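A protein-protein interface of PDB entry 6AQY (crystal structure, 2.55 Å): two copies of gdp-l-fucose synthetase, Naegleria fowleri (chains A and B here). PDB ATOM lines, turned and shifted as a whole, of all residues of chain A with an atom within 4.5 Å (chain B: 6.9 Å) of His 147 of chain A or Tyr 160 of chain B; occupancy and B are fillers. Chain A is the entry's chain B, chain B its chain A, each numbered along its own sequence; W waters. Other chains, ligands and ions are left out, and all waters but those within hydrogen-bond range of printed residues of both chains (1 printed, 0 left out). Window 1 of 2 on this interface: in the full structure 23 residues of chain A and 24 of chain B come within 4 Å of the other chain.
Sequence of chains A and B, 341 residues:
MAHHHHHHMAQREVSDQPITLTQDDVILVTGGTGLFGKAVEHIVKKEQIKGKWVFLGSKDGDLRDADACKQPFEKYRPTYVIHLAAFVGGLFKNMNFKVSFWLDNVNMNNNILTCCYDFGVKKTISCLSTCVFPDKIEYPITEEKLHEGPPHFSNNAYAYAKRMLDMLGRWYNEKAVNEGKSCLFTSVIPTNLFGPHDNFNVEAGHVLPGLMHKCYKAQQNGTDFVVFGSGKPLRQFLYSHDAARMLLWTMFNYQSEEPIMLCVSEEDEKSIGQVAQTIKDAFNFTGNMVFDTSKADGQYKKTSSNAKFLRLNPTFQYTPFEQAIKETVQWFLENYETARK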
ATOM      1  N   LYS A 145      16.376 -21.636 -11.867  1.00  0.00           N
ATOM      2  CA  LYS A 145      14.931 -21.818 -11.863  1.00  0.00           C
ATOM      3  C   LYS A 145      14.188 -20.644 -12.492  1.00  0.00           C
ATOM      4  O   LYS A 145      12.960 -20.646 -12.493  1.00  0.00           O
ATOM      5  CB  LYS A 145      14.439 -22.027 -10.440  1.00  0.00           C
ATOM      6  CG  LYS A 145      15.241 -23.018  -9.657  1.00  0.00           C
ATOM      7  CD  LYS A 145      14.728 -23.070  -8.244  1.00  0.00           C
ATOM      8  CE  LYS A 145      15.227 -24.294  -7.528  1.00  0.00           C
ATOM      9  NZ  LYS A 145      14.698 -24.298  -6.156  1.00  0.00           N
ATOM     10  N   LEU A 146      14.922 -19.675 -13.040  1.00  0.00           N
ATOM     11  CA  LEU A 146      14.347 -18.428 -13.512  1.00  0.00           C
ATOM     12  C   LEU A 146      13.188 -18.639 -14.494  1.00  0.00           C
ATOM     13  O   LEU A 146      12.153 -17.958 -14.410  1.00  0.00           O
ATOM     14  CB  LEU A 146      15.463 -17.610 -14.165  1.00  0.00           C
ATOM     15  CG  LEU A 146      15.062 -16.291 -14.834  1.00  0.00           C
ATOM     16  CD1 LEU A 146      14.395 -15.377 -13.812  1.00  0.00           C
ATOM     17  CD2 LEU A 146      16.257 -15.610 -15.529  1.00  0.00           C
ATOM     18  N   HIS A 147      13.345 -19.558 -15.444  1.00  0.00           N
ATOM     19  CA  HIS A 147      12.335 -19.752 -16.476  1.00  0.00           C
ATOM     20  C   HIS A 147      11.488 -21.005 -16.250  1.00  0.00           C
ATOM     21  O   HIS A 147      10.784 -21.436 -17.169  1.00  0.00           O
ATOM     22  CB  HIS A 147      12.971 -19.788 -17.866  1.00  0.00           C
ATOM     23  CG  HIS A 147      13.705 -18.530 -18.230  1.00  0.00           C
ATOM     24  ND1 HIS A 147      13.059 -17.366 -18.596  1.00  0.00           N
ATOM     25  CD2 HIS A 147      15.030 -18.264 -18.316  1.00  0.00           C
ATOM     26  CE1 HIS A 147      13.952 -16.433 -18.868  1.00  0.00           C
ATOM     27  NE2 HIS A 147      15.154 -16.953 -18.704  1.00  0.00           N
ATOM     28  N   GLU A 148      11.533 -21.600 -15.059  1.00  0.00           N
ATOM     29  CA  GLU A 148      10.837 -22.863 -14.815  1.00  0.00           C
ATOM     30  C   GLU A 148       9.403 -22.614 -14.337  1.00  0.00           C
ATOM     31  O   GLU A 148       8.999 -22.976 -13.236  1.00  0.00           O
ATOM     32  CB  GLU A 148      11.625 -23.705 -13.822  1.00  0.00           C
ATOM     33  CG  GLU A 148      12.973 -24.153 -14.369  1.00  0.00           C
ATOM     34  CD  GLU A 148      12.868 -25.027 -15.616  1.00  0.00           C
ATOM     35  OE1 GLU A 148      11.971 -25.902 -15.706  1.00  0.00           O
ATOM     36  OE2 GLU A 148      13.692 -24.818 -16.526  1.00  0.00           O
ATOM     37  N   GLY A 149       8.617 -21.977 -15.196  1.00  0.00           N
ATOM     38  CA  GLY A 149       7.235 -21.753 -14.871  1.00  0.00           C
ATOM     39  C   GLY A 149       6.844 -20.294 -14.777  1.00  0.00           C
ATOM     40  O   GLY A 149       7.691 -19.396 -14.762  1.00  0.00           O
ATOM     41  N   ARG A 163      12.422 -11.507 -17.602  1.00  0.00           N
ATOM     42  CA  ARG A 163      12.763 -12.805 -18.184  1.00  0.00           C
ATOM     43  C   ARG A 163      13.202 -12.685 -19.649  1.00  0.00           C
ATOM     44  O   ARG A 163      14.048 -13.463 -20.119  1.00  0.00           O
ATOM     45  CB  ARG A 163      11.560 -13.744 -18.075  1.00  0.00           C
ATOM     46  CG  ARG A 163      11.092 -13.966 -16.632  1.00  0.00           C
ATOM     47  CD  ARG A 163      10.602 -15.321 -16.525  1.00  0.00           C
ATOM     48  NE  ARG A 163      10.080 -15.643 -15.220  1.00  0.00           N
ATOM     49  CZ  ARG A 163       9.330 -16.716 -15.021  1.00  0.00           C
ATOM     50  NH1 ARG A 163       9.060 -17.492 -16.065  1.00  0.00           N
ATOM     51  NH2 ARG A 163       8.843 -17.007 -13.817  1.00  0.00           N
ATOM     52  N   MET A 164      12.551 -11.799 -20.413  1.00  0.00           N
ATOM     53  CA  MET A 164      12.928 -11.577 -21.798  1.00  0.00           C
ATOM     54  C   MET A 164      14.152 -10.680 -21.945  1.00  0.00           C
ATOM     55  O   MET A 164      14.755 -10.652 -23.021  1.00  0.00           O
ATOM     56  CB  MET A 164      11.754 -10.994 -22.562  1.00  0.00           C
ATOM     57  CG  MET A 164      10.579 -11.979 -22.664  1.00  0.00           C
ATOM     58  SD  MET A 164      11.027 -13.594 -23.286  1.00  0.00           S
ATOM     59  CE  MET A 164      10.952 -14.603 -21.850  1.00  0.00           C
ATOM     60  N   ASP A 166      16.759 -11.195 -19.842  1.00  0.00           N
ATOM     61  CA  ASP A 166      17.734 -12.280 -19.730  1.00  0.00           C
ATOM     62  C   ASP A 166      17.901 -13.028 -21.057  1.00  0.00           C
ATOM     63  O   ASP A 166      19.029 -13.232 -21.527  1.00  0.00           O
ATOM     64  CB  ASP A 166      17.320 -13.246 -18.605  1.00  0.00           C
ATOM     65  CG  ASP A 166      18.216 -14.495 -18.533  1.00  0.00           C
ATOM     66  OD1 ASP A 166      19.416 -14.361 -18.220  1.00  0.00           O
ATOM     67  OD2 ASP A 166      17.732 -15.616 -18.777  1.00  0.00           O
ATOM     68  N   MET A 167      16.788 -13.453 -21.676  1.00  0.00           N
ATOM     69  CA  MET A 167      16.853 -14.211 -22.927  1.00  0.00           C
ATOM     70  C   MET A 167      17.490 -13.388 -24.049  1.00  0.00           C
ATOM     71  O   MET A 167      18.337 -13.891 -24.794  1.00  0.00           O
ATOM     72  CB  MET A 167      15.451 -14.678 -23.328  1.00  0.00           C
ATOM     73  CG  MET A 167      14.787 -15.701 -22.384  1.00  0.00           C
ATOM     74  SD  MET A 167      15.713 -17.236 -22.094  1.00  0.00           S
ATOM     75  CE  MET A 167      15.926 -17.788 -23.766  1.00  0.00           C
ATOM     76  N   TRP A 171      20.583 -14.402 -26.466  1.00  0.00           N
ATOM     77  CA  TRP A 171      20.472 -14.419 -27.921  1.00  0.00           C
ATOM     78  C   TRP A 171      21.501 -13.493 -28.568  1.00  0.00           C
ATOM     79  O   TRP A 171      22.025 -13.808 -29.644  1.00  0.00           O
ATOM     80  CB  TRP A 171      19.050 -14.053 -28.358  1.00  0.00           C
ATOM     81  CG  TRP A 171      18.041 -15.070 -27.935  1.00  0.00           C
ATOM     82  CD1 TRP A 171      18.246 -16.405 -27.791  1.00  0.00           C
ATOM     83  CD2 TRP A 171      16.669 -14.836 -27.588  1.00  0.00           C
ATOM     84  NE1 TRP A 171      17.093 -17.023 -27.384  1.00  0.00           N
ATOM     85  CE2 TRP A 171      16.108 -16.084 -27.250  1.00  0.00           C
ATOM     86  CE3 TRP A 171      15.863 -13.694 -27.532  1.00  0.00           C
ATOM     87  CZ2 TRP A 171      14.779 -16.230 -26.862  1.00  0.00           C
ATOM     88  CZ3 TRP A 171      14.538 -13.841 -27.157  1.00  0.00           C
ATOM     89  CH2 TRP A 171      14.012 -15.100 -26.823  1.00  0.00           C
ATOM     90  N   TRP B 102      13.115 -12.721 -32.226  1.00  0.00           N
ATOM     91  CA  TRP B 102      12.503 -12.092 -31.070  1.00  0.00           C
ATOM     92  C   TRP B 102      12.026 -10.685 -31.410  1.00  0.00           C
ATOM     93  O   TRP B 102      10.846 -10.354 -31.217  1.00  0.00           O
ATOM     94  CB  TRP B 102      13.488 -12.072 -29.898  1.00  0.00           C
ATOM     95  CG  TRP B 102      13.031 -11.145 -28.825  1.00  0.00           C
ATOM     96  CD1 TRP B 102      13.561  -9.933 -28.512  1.00  0.00           C
ATOM     97  CD2 TRP B 102      11.908 -11.337 -27.948  1.00  0.00           C
ATOM     98  NE1 TRP B 102      12.847  -9.358 -27.486  1.00  0.00           N
ATOM     99  CE2 TRP B 102      11.822 -10.198 -27.128  1.00  0.00           C
ATOM    100  CE3 TRP B 102      10.959 -12.364 -27.787  1.00  0.00           C
ATOM    101  CZ2 TRP B 102      10.833 -10.055 -26.145  1.00  0.00           C
ATOM    102  CZ3 TRP B 102       9.980 -12.217 -26.818  1.00  0.00           C
ATOM    103  CH2 TRP B 102       9.918 -11.070 -26.012  1.00  0.00           C
ATOM    104  N   VAL B 106       8.045  -9.726 -31.705  1.00  0.00           N
ATOM    105  CA  VAL B 106       7.507  -9.012 -30.545  1.00  0.00           C
ATOM    106  C   VAL B 106       7.126  -7.580 -30.923  1.00  0.00           C
ATOM    107  O   VAL B 106       6.134  -7.043 -30.409  1.00  0.00           O
ATOM    108  CB  VAL B 106       8.463  -9.056 -29.332  1.00  0.00           C
ATOM    109  CG1 VAL B 106       9.634  -8.029 -29.434  1.00  0.00           C
ATOM    110  CG2 VAL B 106       7.662  -8.783 -28.078  1.00  0.00           C
ATOM    111  N   ASN B 109       3.843  -7.862 -32.945  1.00  0.00           N
ATOM    112  CA  ASN B 109       2.770  -8.242 -32.033  1.00  0.00           C
ATOM    113  C   ASN B 109       2.377  -7.082 -31.121  1.00  0.00           C
ATOM    114  O   ASN B 109       1.181  -6.873 -30.862  1.00  0.00           O
ATOM    115  CB  ASN B 109       3.178  -9.452 -31.202  1.00  0.00           C
ATOM    116  CG  ASN B 109       3.214 -10.717 -31.999  1.00  0.00           C
ATOM    117  OD1 ASN B 109       2.543 -10.839 -33.029  1.00  0.00           O
ATOM    118  ND2 ASN B 109       4.051 -11.660 -31.564  1.00  0.00           N
ATOM    119  N   VAL B 132       5.418 -23.772 -29.455  1.00  0.00           N
ATOM    120  CA  VAL B 132       5.726 -22.870 -28.348  1.00  0.00           C
ATOM    121  C   VAL B 132       5.408 -23.471 -26.979  1.00  0.00           C
ATOM    122  O   VAL B 132       5.625 -22.813 -25.961  1.00  0.00           O
ATOM    123  CB  VAL B 132       4.981 -21.533 -28.521  1.00  0.00           C
ATOM    124  CG1 VAL B 132       5.168 -21.032 -29.945  1.00  0.00           C
ATOM    125  CG2 VAL B 132       3.490 -21.657 -28.166  1.00  0.00           C
ATOM    126  N   HIS B 147       2.364 -22.011 -20.610  1.00  0.00           N
ATOM    127  CA  HIS B 147       3.449 -21.284 -19.959  1.00  0.00           C
ATOM    128  C   HIS B 147       4.158 -22.100 -18.895  1.00  0.00           C
ATOM    129  O   HIS B 147       4.940 -21.545 -18.122  1.00  0.00           O
ATOM    130  CB  HIS B 147       2.919 -20.011 -19.299  1.00  0.00           C
ATOM    131  CG  HIS B 147       2.300 -19.048 -20.251  1.00  0.00           C
ATOM    132  ND1 HIS B 147       3.046 -18.188 -21.036  1.00  0.00           N
ATOM    133  CD2 HIS B 147       1.003 -18.825 -20.569  1.00  0.00           C
ATOM    134  CE1 HIS B 147       2.227 -17.467 -21.783  1.00  0.00           C
ATOM    135  NE2 HIS B 147       0.985 -17.834 -21.521  1.00  0.00           N
ATOM    136  N   GLU B 148       3.916 -23.396 -18.835  1.00  0.00           N
ATOM    137  CA  GLU B 148       4.409 -24.211 -17.727  1.00  0.00           C
ATOM    138  C   GLU B 148       5.825 -24.707 -18.018  1.00  0.00           C
ATOM    139  O   GLU B 148       6.085 -25.902 -18.119  1.00  0.00           O
ATOM    140  CB  GLU B 148       3.448 -25.370 -17.497  1.00  0.00           C
ATOM    141  CG  GLU B 148       2.075 -24.952 -17.035  1.00  0.00           C
ATOM    142  CD  GLU B 148       2.107 -24.264 -15.674  1.00  0.00           C
ATOM    143  OE1 GLU B 148       2.873 -24.710 -14.791  1.00  0.00           O
ATOM    144  OE2 GLU B 148       1.378 -23.269 -15.485  1.00  0.00           O
ATOM    145  N   GLY B 149       6.753 -23.761 -18.178  1.00  0.00           N
ATOM    146  CA  GLY B 149       8.129 -24.119 -18.406  1.00  0.00           C
ATOM    147  C   GLY B 149       8.672 -23.667 -19.744  1.00  0.00           C
ATOM    148  O   GLY B 149       7.934 -23.229 -20.631  1.00  0.00           O
ATOM    149  N   PRO B 150       9.992 -23.769 -19.913  1.00  0.00           N
ATOM    150  CA  PRO B 150      10.621 -23.180 -21.092  1.00  0.00           C
ATOM    151  C   PRO B 150      10.324 -24.001 -22.336  1.00  0.00           C
ATOM    152  O   PRO B 150      10.139 -25.224 -22.256  1.00  0.00           O
ATOM    153  CB  PRO B 150      12.123 -23.211 -20.747  1.00  0.00           C
ATOM    154  CG  PRO B 150      12.259 -24.302 -19.781  1.00  0.00           C
ATOM    155  CD  PRO B 150      10.987 -24.309 -18.967  1.00  0.00           C
ATOM    156  N   PRO B 151      10.252 -23.355 -23.521  1.00  0.00           N
ATOM    157  CA  PRO B 151      10.131 -24.099 -24.795  1.00  0.00           C
ATOM    158  C   PRO B 151      11.422 -24.770 -25.213  1.00  0.00           C
ATOM    159  O   PRO B 151      12.425 -24.633 -24.511  1.00  0.00           O
ATOM    160  CB  PRO B 151       9.751 -23.007 -25.793  1.00  0.00           C
ATOM    161  CG  PRO B 151      10.370 -21.778 -25.215  1.00  0.00           C
ATOM    162  CD  PRO B 151      10.264 -21.899 -23.729  1.00  0.00           C
ATOM    163  N   ASN B 155      13.847 -23.139 -31.296  1.00  0.00           N
ATOM    164  CA  ASN B 155      13.033 -22.030 -31.798  1.00  0.00           C
ATOM    165  C   ASN B 155      12.502 -21.157 -30.663  1.00  0.00           C
ATOM    166  O   ASN B 155      11.398 -20.594 -30.741  1.00  0.00           O
ATOM    167  CB  ASN B 155      11.866 -22.550 -32.639  1.00  0.00           C
ATOM    168  N   ASN B 156      13.299 -20.988 -29.608  1.00  0.00           N
ATOM    169  CA  ASN B 156      12.745 -20.368 -28.412  1.00  0.00           C
ATOM    170  C   ASN B 156      12.553 -18.861 -28.533  1.00  0.00           C
ATOM    171  O   ASN B 156      11.791 -18.292 -27.744  1.00  0.00           O
ATOM    172  CB  ASN B 156      13.589 -20.717 -27.184  1.00  0.00           C
ATOM    173  CG  ASN B 156      15.035 -20.266 -27.297  1.00  0.00           C
ATOM    174  OD1 ASN B 156      15.476 -19.671 -28.297  1.00  0.00           O
ATOM    175  ND2 ASN B 156      15.793 -20.583 -26.269  1.00  0.00           N
ATOM    176  N   ALA B 157      13.223 -18.185 -29.470  1.00  0.00           N
ATOM    177  CA  ALA B 157      12.920 -16.770 -29.670  1.00  0.00           C
ATOM    178  C   ALA B 157      11.528 -16.611 -30.267  1.00  0.00           C
ATOM    179  O   ALA B 157      10.670 -15.904 -29.708  1.00  0.00           O
ATOM    180  CB  ALA B 157      13.977 -16.117 -30.557  1.00  0.00           C
ATOM    181  N   TYR B 158      11.264 -17.349 -31.353  1.00  0.00           N
ATOM    182  CA  TYR B 158       9.924 -17.386 -31.925  1.00  0.00           C
ATOM    183  C   TYR B 158       8.902 -17.877 -30.897  1.00  0.00           C
ATOM    184  O   TYR B 158       7.798 -17.338 -30.791  1.00  0.00           O
ATOM    185  CB  TYR B 158       9.927 -18.281 -33.164  1.00  0.00           C
ATOM    186  CG  TYR B 158       8.565 -18.526 -33.752  1.00  0.00           C
ATOM    187  CD1 TYR B 158       7.753 -19.558 -33.279  1.00  0.00           C
ATOM    188  CD2 TYR B 158       8.089 -17.731 -34.789  1.00  0.00           C
ATOM    189  CE1 TYR B 158       6.513 -19.788 -33.807  1.00  0.00           C
ATOM    190  CE2 TYR B 158       6.831 -17.948 -35.326  1.00  0.00           C
ATOM    191  CZ  TYR B 158       6.041 -18.984 -34.824  1.00  0.00           C
ATOM    192  OH  TYR B 158       4.786 -19.228 -35.345  1.00  0.00           O
ATOM    193  N   ALA B 159       9.270 -18.888 -30.116  1.00  0.00           N
ATOM    194  CA  ALA B 159       8.355 -19.445 -29.131  1.00  0.00           C
ATOM    195  C   ALA B 159       7.956 -18.403 -28.104  1.00  0.00           C
ATOM    196  O   ALA B 159       6.773 -18.273 -27.766  1.00  0.00           O
ATOM    197  CB  ALA B 159       8.997 -20.647 -28.444  1.00  0.00           C
ATOM    198  N   TYR B 160       8.944 -17.685 -27.554  1.00  0.00           N
ATOM    199  CA  TYR B 160       8.645 -16.715 -26.511  1.00  0.00           C
ATOM    200  C   TYR B 160       7.861 -15.529 -27.052  1.00  0.00           C
ATOM    201  O   TYR B 160       6.965 -15.024 -26.367  1.00  0.00           O
ATOM    202  CB  TYR B 160       9.925 -16.257 -25.828  1.00  0.00           C
ATOM    203  CG  TYR B 160      10.325 -17.131 -24.672  1.00  0.00           C
ATOM    204  CD1 TYR B 160       9.453 -17.342 -23.593  1.00  0.00           C
ATOM    205  CD2 TYR B 160      11.571 -17.755 -24.655  1.00  0.00           C
ATOM    206  CE1 TYR B 160       9.821 -18.156 -22.527  1.00  0.00           C
ATOM    207  CE2 TYR B 160      11.938 -18.563 -23.615  1.00  0.00           C
ATOM    208  CZ  TYR B 160      11.071 -18.762 -22.546  1.00  0.00           C
ATOM    209  OH  TYR B 160      11.481 -19.578 -21.511  1.00  0.00           O
ATOM    210  N   ALA B 161       8.165 -15.067 -28.274  1.00  0.00           N
ATOM    211  CA  ALA B 161       7.326 -14.009 -28.843  1.00  0.00           C
ATOM    212  C   ALA B 161       5.873 -14.449 -28.903  1.00  0.00           C
ATOM    213  O   ALA B 161       4.982 -13.651 -28.613  1.00  0.00           O
ATOM    214  CB  ALA B 161       7.792 -13.563 -30.228  1.00  0.00           C
ATOM    215  N   LYS B 162       5.614 -15.710 -29.281  1.00  0.00           N
ATOM    216  CA  LYS B 162       4.232 -16.193 -29.295  1.00  0.00           C
ATOM    217  C   LYS B 162       3.633 -16.211 -27.897  1.00  0.00           C
ATOM    218  O   LYS B 162       2.477 -15.803 -27.704  1.00  0.00           O
ATOM    219  CB  LYS B 162       4.147 -17.582 -29.910  1.00  0.00           C
ATOM    220  CG  LYS B 162       4.266 -17.600 -31.411  1.00  0.00           C
ATOM    221  CD  LYS B 162       3.248 -16.705 -32.043  1.00  0.00           C
ATOM    222  CE  LYS B 162       3.208 -16.967 -33.539  1.00  0.00           C
ATOM    223  NZ  LYS B 162       2.197 -16.124 -34.134  1.00  0.00           N
ATOM    224  N   ARG B 163       4.412 -16.672 -26.915  1.00  0.00           N
ATOM    225  CA  ARG B 163       3.959 -16.676 -25.530  1.00  0.00           C
ATOM    226  C   ARG B 163       3.611 -15.276 -25.049  1.00  0.00           C
ATOM    227  O   ARG B 163       2.635 -15.104 -24.317  1.00  0.00           O
ATOM    228  CB  ARG B 163       5.041 -17.272 -24.618  1.00  0.00           C
ATOM    229  CG  ARG B 163       5.412 -18.684 -24.946  1.00  0.00           C
ATOM    230  CD  ARG B 163       5.672 -19.465 -23.674  1.00  0.00           C
ATOM    231  NE  ARG B 163       6.010 -20.858 -23.936  1.00  0.00           N
ATOM    232  CZ  ARG B 163       6.520 -21.669 -23.027  1.00  0.00           C
ATOM    233  NH1 ARG B 163       6.743 -21.206 -21.794  1.00  0.00           N
ATOM    234  NH2 ARG B 163       6.790 -22.934 -23.345  1.00  0.00           N
ATOM    235  N   MET B 164       4.424 -14.268 -25.415  1.00  0.00           N
ATOM    236  CA  MET B 164       4.162 -12.889 -25.019  1.00  0.00           C
ATOM    237  C   MET B 164       3.067 -12.241 -25.857  1.00  0.00           C
ATOM    238  O   MET B 164       2.455 -11.273 -25.403  1.00  0.00           O
ATOM    239  CB  MET B 164       5.443 -12.058 -25.097  1.00  0.00           C
ATOM    240  CG  MET B 164       6.531 -12.545 -24.120  1.00  0.00           C
ATOM    241  SD  MET B 164       5.943 -12.696 -22.422  1.00  0.00           S
ATOM    242  CE  MET B 164       5.788 -14.475 -22.248  1.00  0.00           C
ATOM    243  N   LEU B 165       2.788 -12.768 -27.049  1.00  0.00           N
ATOM    244  CA  LEU B 165       1.594 -12.356 -27.766  1.00  0.00           C
ATOM    245  C   LEU B 165       0.340 -12.753 -26.984  1.00  0.00           C
ATOM    246  O   LEU B 165      -0.606 -11.962 -26.858  1.00  0.00           O
ATOM    247  CB  LEU B 165       1.575 -12.987 -29.160  1.00  0.00           C
ATOM    248  CG  LEU B 165       0.262 -12.885 -29.979  1.00  0.00           C
ATOM    249  CD1 LEU B 165      -0.164 -11.428 -30.286  1.00  0.00           C
ATOM    250  CD2 LEU B 165       0.469 -13.617 -31.250  1.00  0.00           C
ATOM    251  N   ASP B 166       0.339 -13.976 -26.436  1.00  0.00           N
ATOM    252  CA  ASP B 166      -0.757 -14.455 -25.596  1.00  0.00           C
ATOM    253  C   ASP B 166      -0.927 -13.564 -24.371  1.00  0.00           C
ATOM    254  O   ASP B 166      -2.027 -13.061 -24.110  1.00  0.00           O
ATOM    255  CB  ASP B 166      -0.494 -15.920 -25.197  1.00  0.00           C
ATOM    256  CG  ASP B 166      -1.500 -16.458 -24.212  1.00  0.00           C
ATOM    257  OD1 ASP B 166      -2.655 -16.665 -24.594  1.00  0.00           O
ATOM    258  OD2 ASP B 166      -1.162 -16.594 -23.023  1.00  0.00           O
HETATM  259  O   HOH W   1       9.053 -20.299 -19.471  1.00  0.00           O
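Water W1 lies within hydrogen-bond range of O of His 147 of chain A, OH of Tyr 160 of chain B, O of Gly 149 of chain B and NH1 of Arg 163 of chain B.
OD1 of Asn 156 of chain B is in hydrogen-bond range of NE1 of Trp 171 of chain A (3.2 Å).
His 147 of chain A touches just these residues of chain B: Gly 149 (3.97 Å), Pro 150 (3.4 Å) and Tyr 160 (3.9 Å).
Of chain A, only His 147 and Met 164 come within 4 Å of Tyr 160 of chain B.
Printed residues of chain B within 4 Å of Met 164 of chain A: Trp 102 (3.5 Å) and Tyr 160 (3.6 Å).
Of the printed residues of chain A, Ala 157 of chain B touches Trp 171 (3.4 Å).
Of the printed residues of chain B, Trp 171 of chain A touches Trp 102, Asn 156 and Ala 157.
Of the printed residues of chain A, Pro 150 of chain B touches His 147 and Glu 148.
Asp 166 of chain A touches none of the printed residues of chain B.
The nearest residue of chain B that does not touch His 147 of chain A is His 147 of chain B (5.9 Å).
The nearest residue of chain A that does not touch Tyr 160 of chain B is Met 167 of chain A (4.1 Å).
His 147 of chain A touches Gly 149 of chain B, and with the chains exchanged Gly 149 of chain A touches His 147 of chain B.
Gly 149 of chain A touches its own counterpart, Gly 149 of chain B.
Positions printed for both chains: 147, 148, 149, 163, 164 and 166.
Among the printed residues, pairs that only touch across the chains: His 147 of chain A with Pro 150 of chain B (3.4 Å), Trp 171 of chain A with Ala 157 of chain B (3.4 Å), Trp 171 of chain A with Trp 102 of chain B (3.4 Å), Met 164 of chain A with Trp 102 of chain B (3.5 Å), Met 164 of chain A with Tyr 160 of chain B (3.6 Å), Glu 148 of chain A with Pro 150 of chain B (3.6 Å), Met 167 of chain A with Asn 156 of chain B (3.8 Å), Gly 149 of chain A with Gly 149 of chain B (3.9 Å), His 147 of chain A with Tyr 160 of chain B (3.9 Å), His 147 of chain A with Gly 149 of chain B (3.97 Å) and Gly 149 of chain A with His 147 of chain B (3.98 Å).
Of the 10 printed residues of chain A, 6 touch a printed residue of chain B.
Hydrophobic or aromatic side chains of chain A within 4 Å of the printed part of chain B: His 147, Met 164, Met 167 and Trp 171.
Of the 21 printed residues of chain B, 7 touch a printed residue of chain A.
Hydrophobic or aromatic side chains of chain B that line the printed part of chain A: Trp 102, Pro 150, Ala 157 and Tyr 160.
Among the printed residues, 12 pairs touch across the chains.
Among the printed residues, no Asp or Glu carboxylate lies within 4 Å of a Lys or Arg side-chain nitrogen of the other chain.
NE2 of His 147 of chain B sits at hydrogen-bond distance from OD2 of Asp 166 of chain B, at 2.9 Å.
The backbone carbonyl oxygen (O) of Gly 149 of chain B sits at hydrogen-bond distance from the guanidinium group (NH1) of Arg 163 of chain B, 2.6 Å away.
NE2 of His 147 of chain A sits at hydrogen-bond distance from OD2 of Asp 166 of chain A (2.9 Å).
NE2 of His 147 of chain A lies within hydrogen-bond range of SD of Met 167 of chain A, at 3.4 Å.
O of Gly 149 of chain A is in hydrogen-bond range of NH1 of Arg 163 of chain A (2.7 Å).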
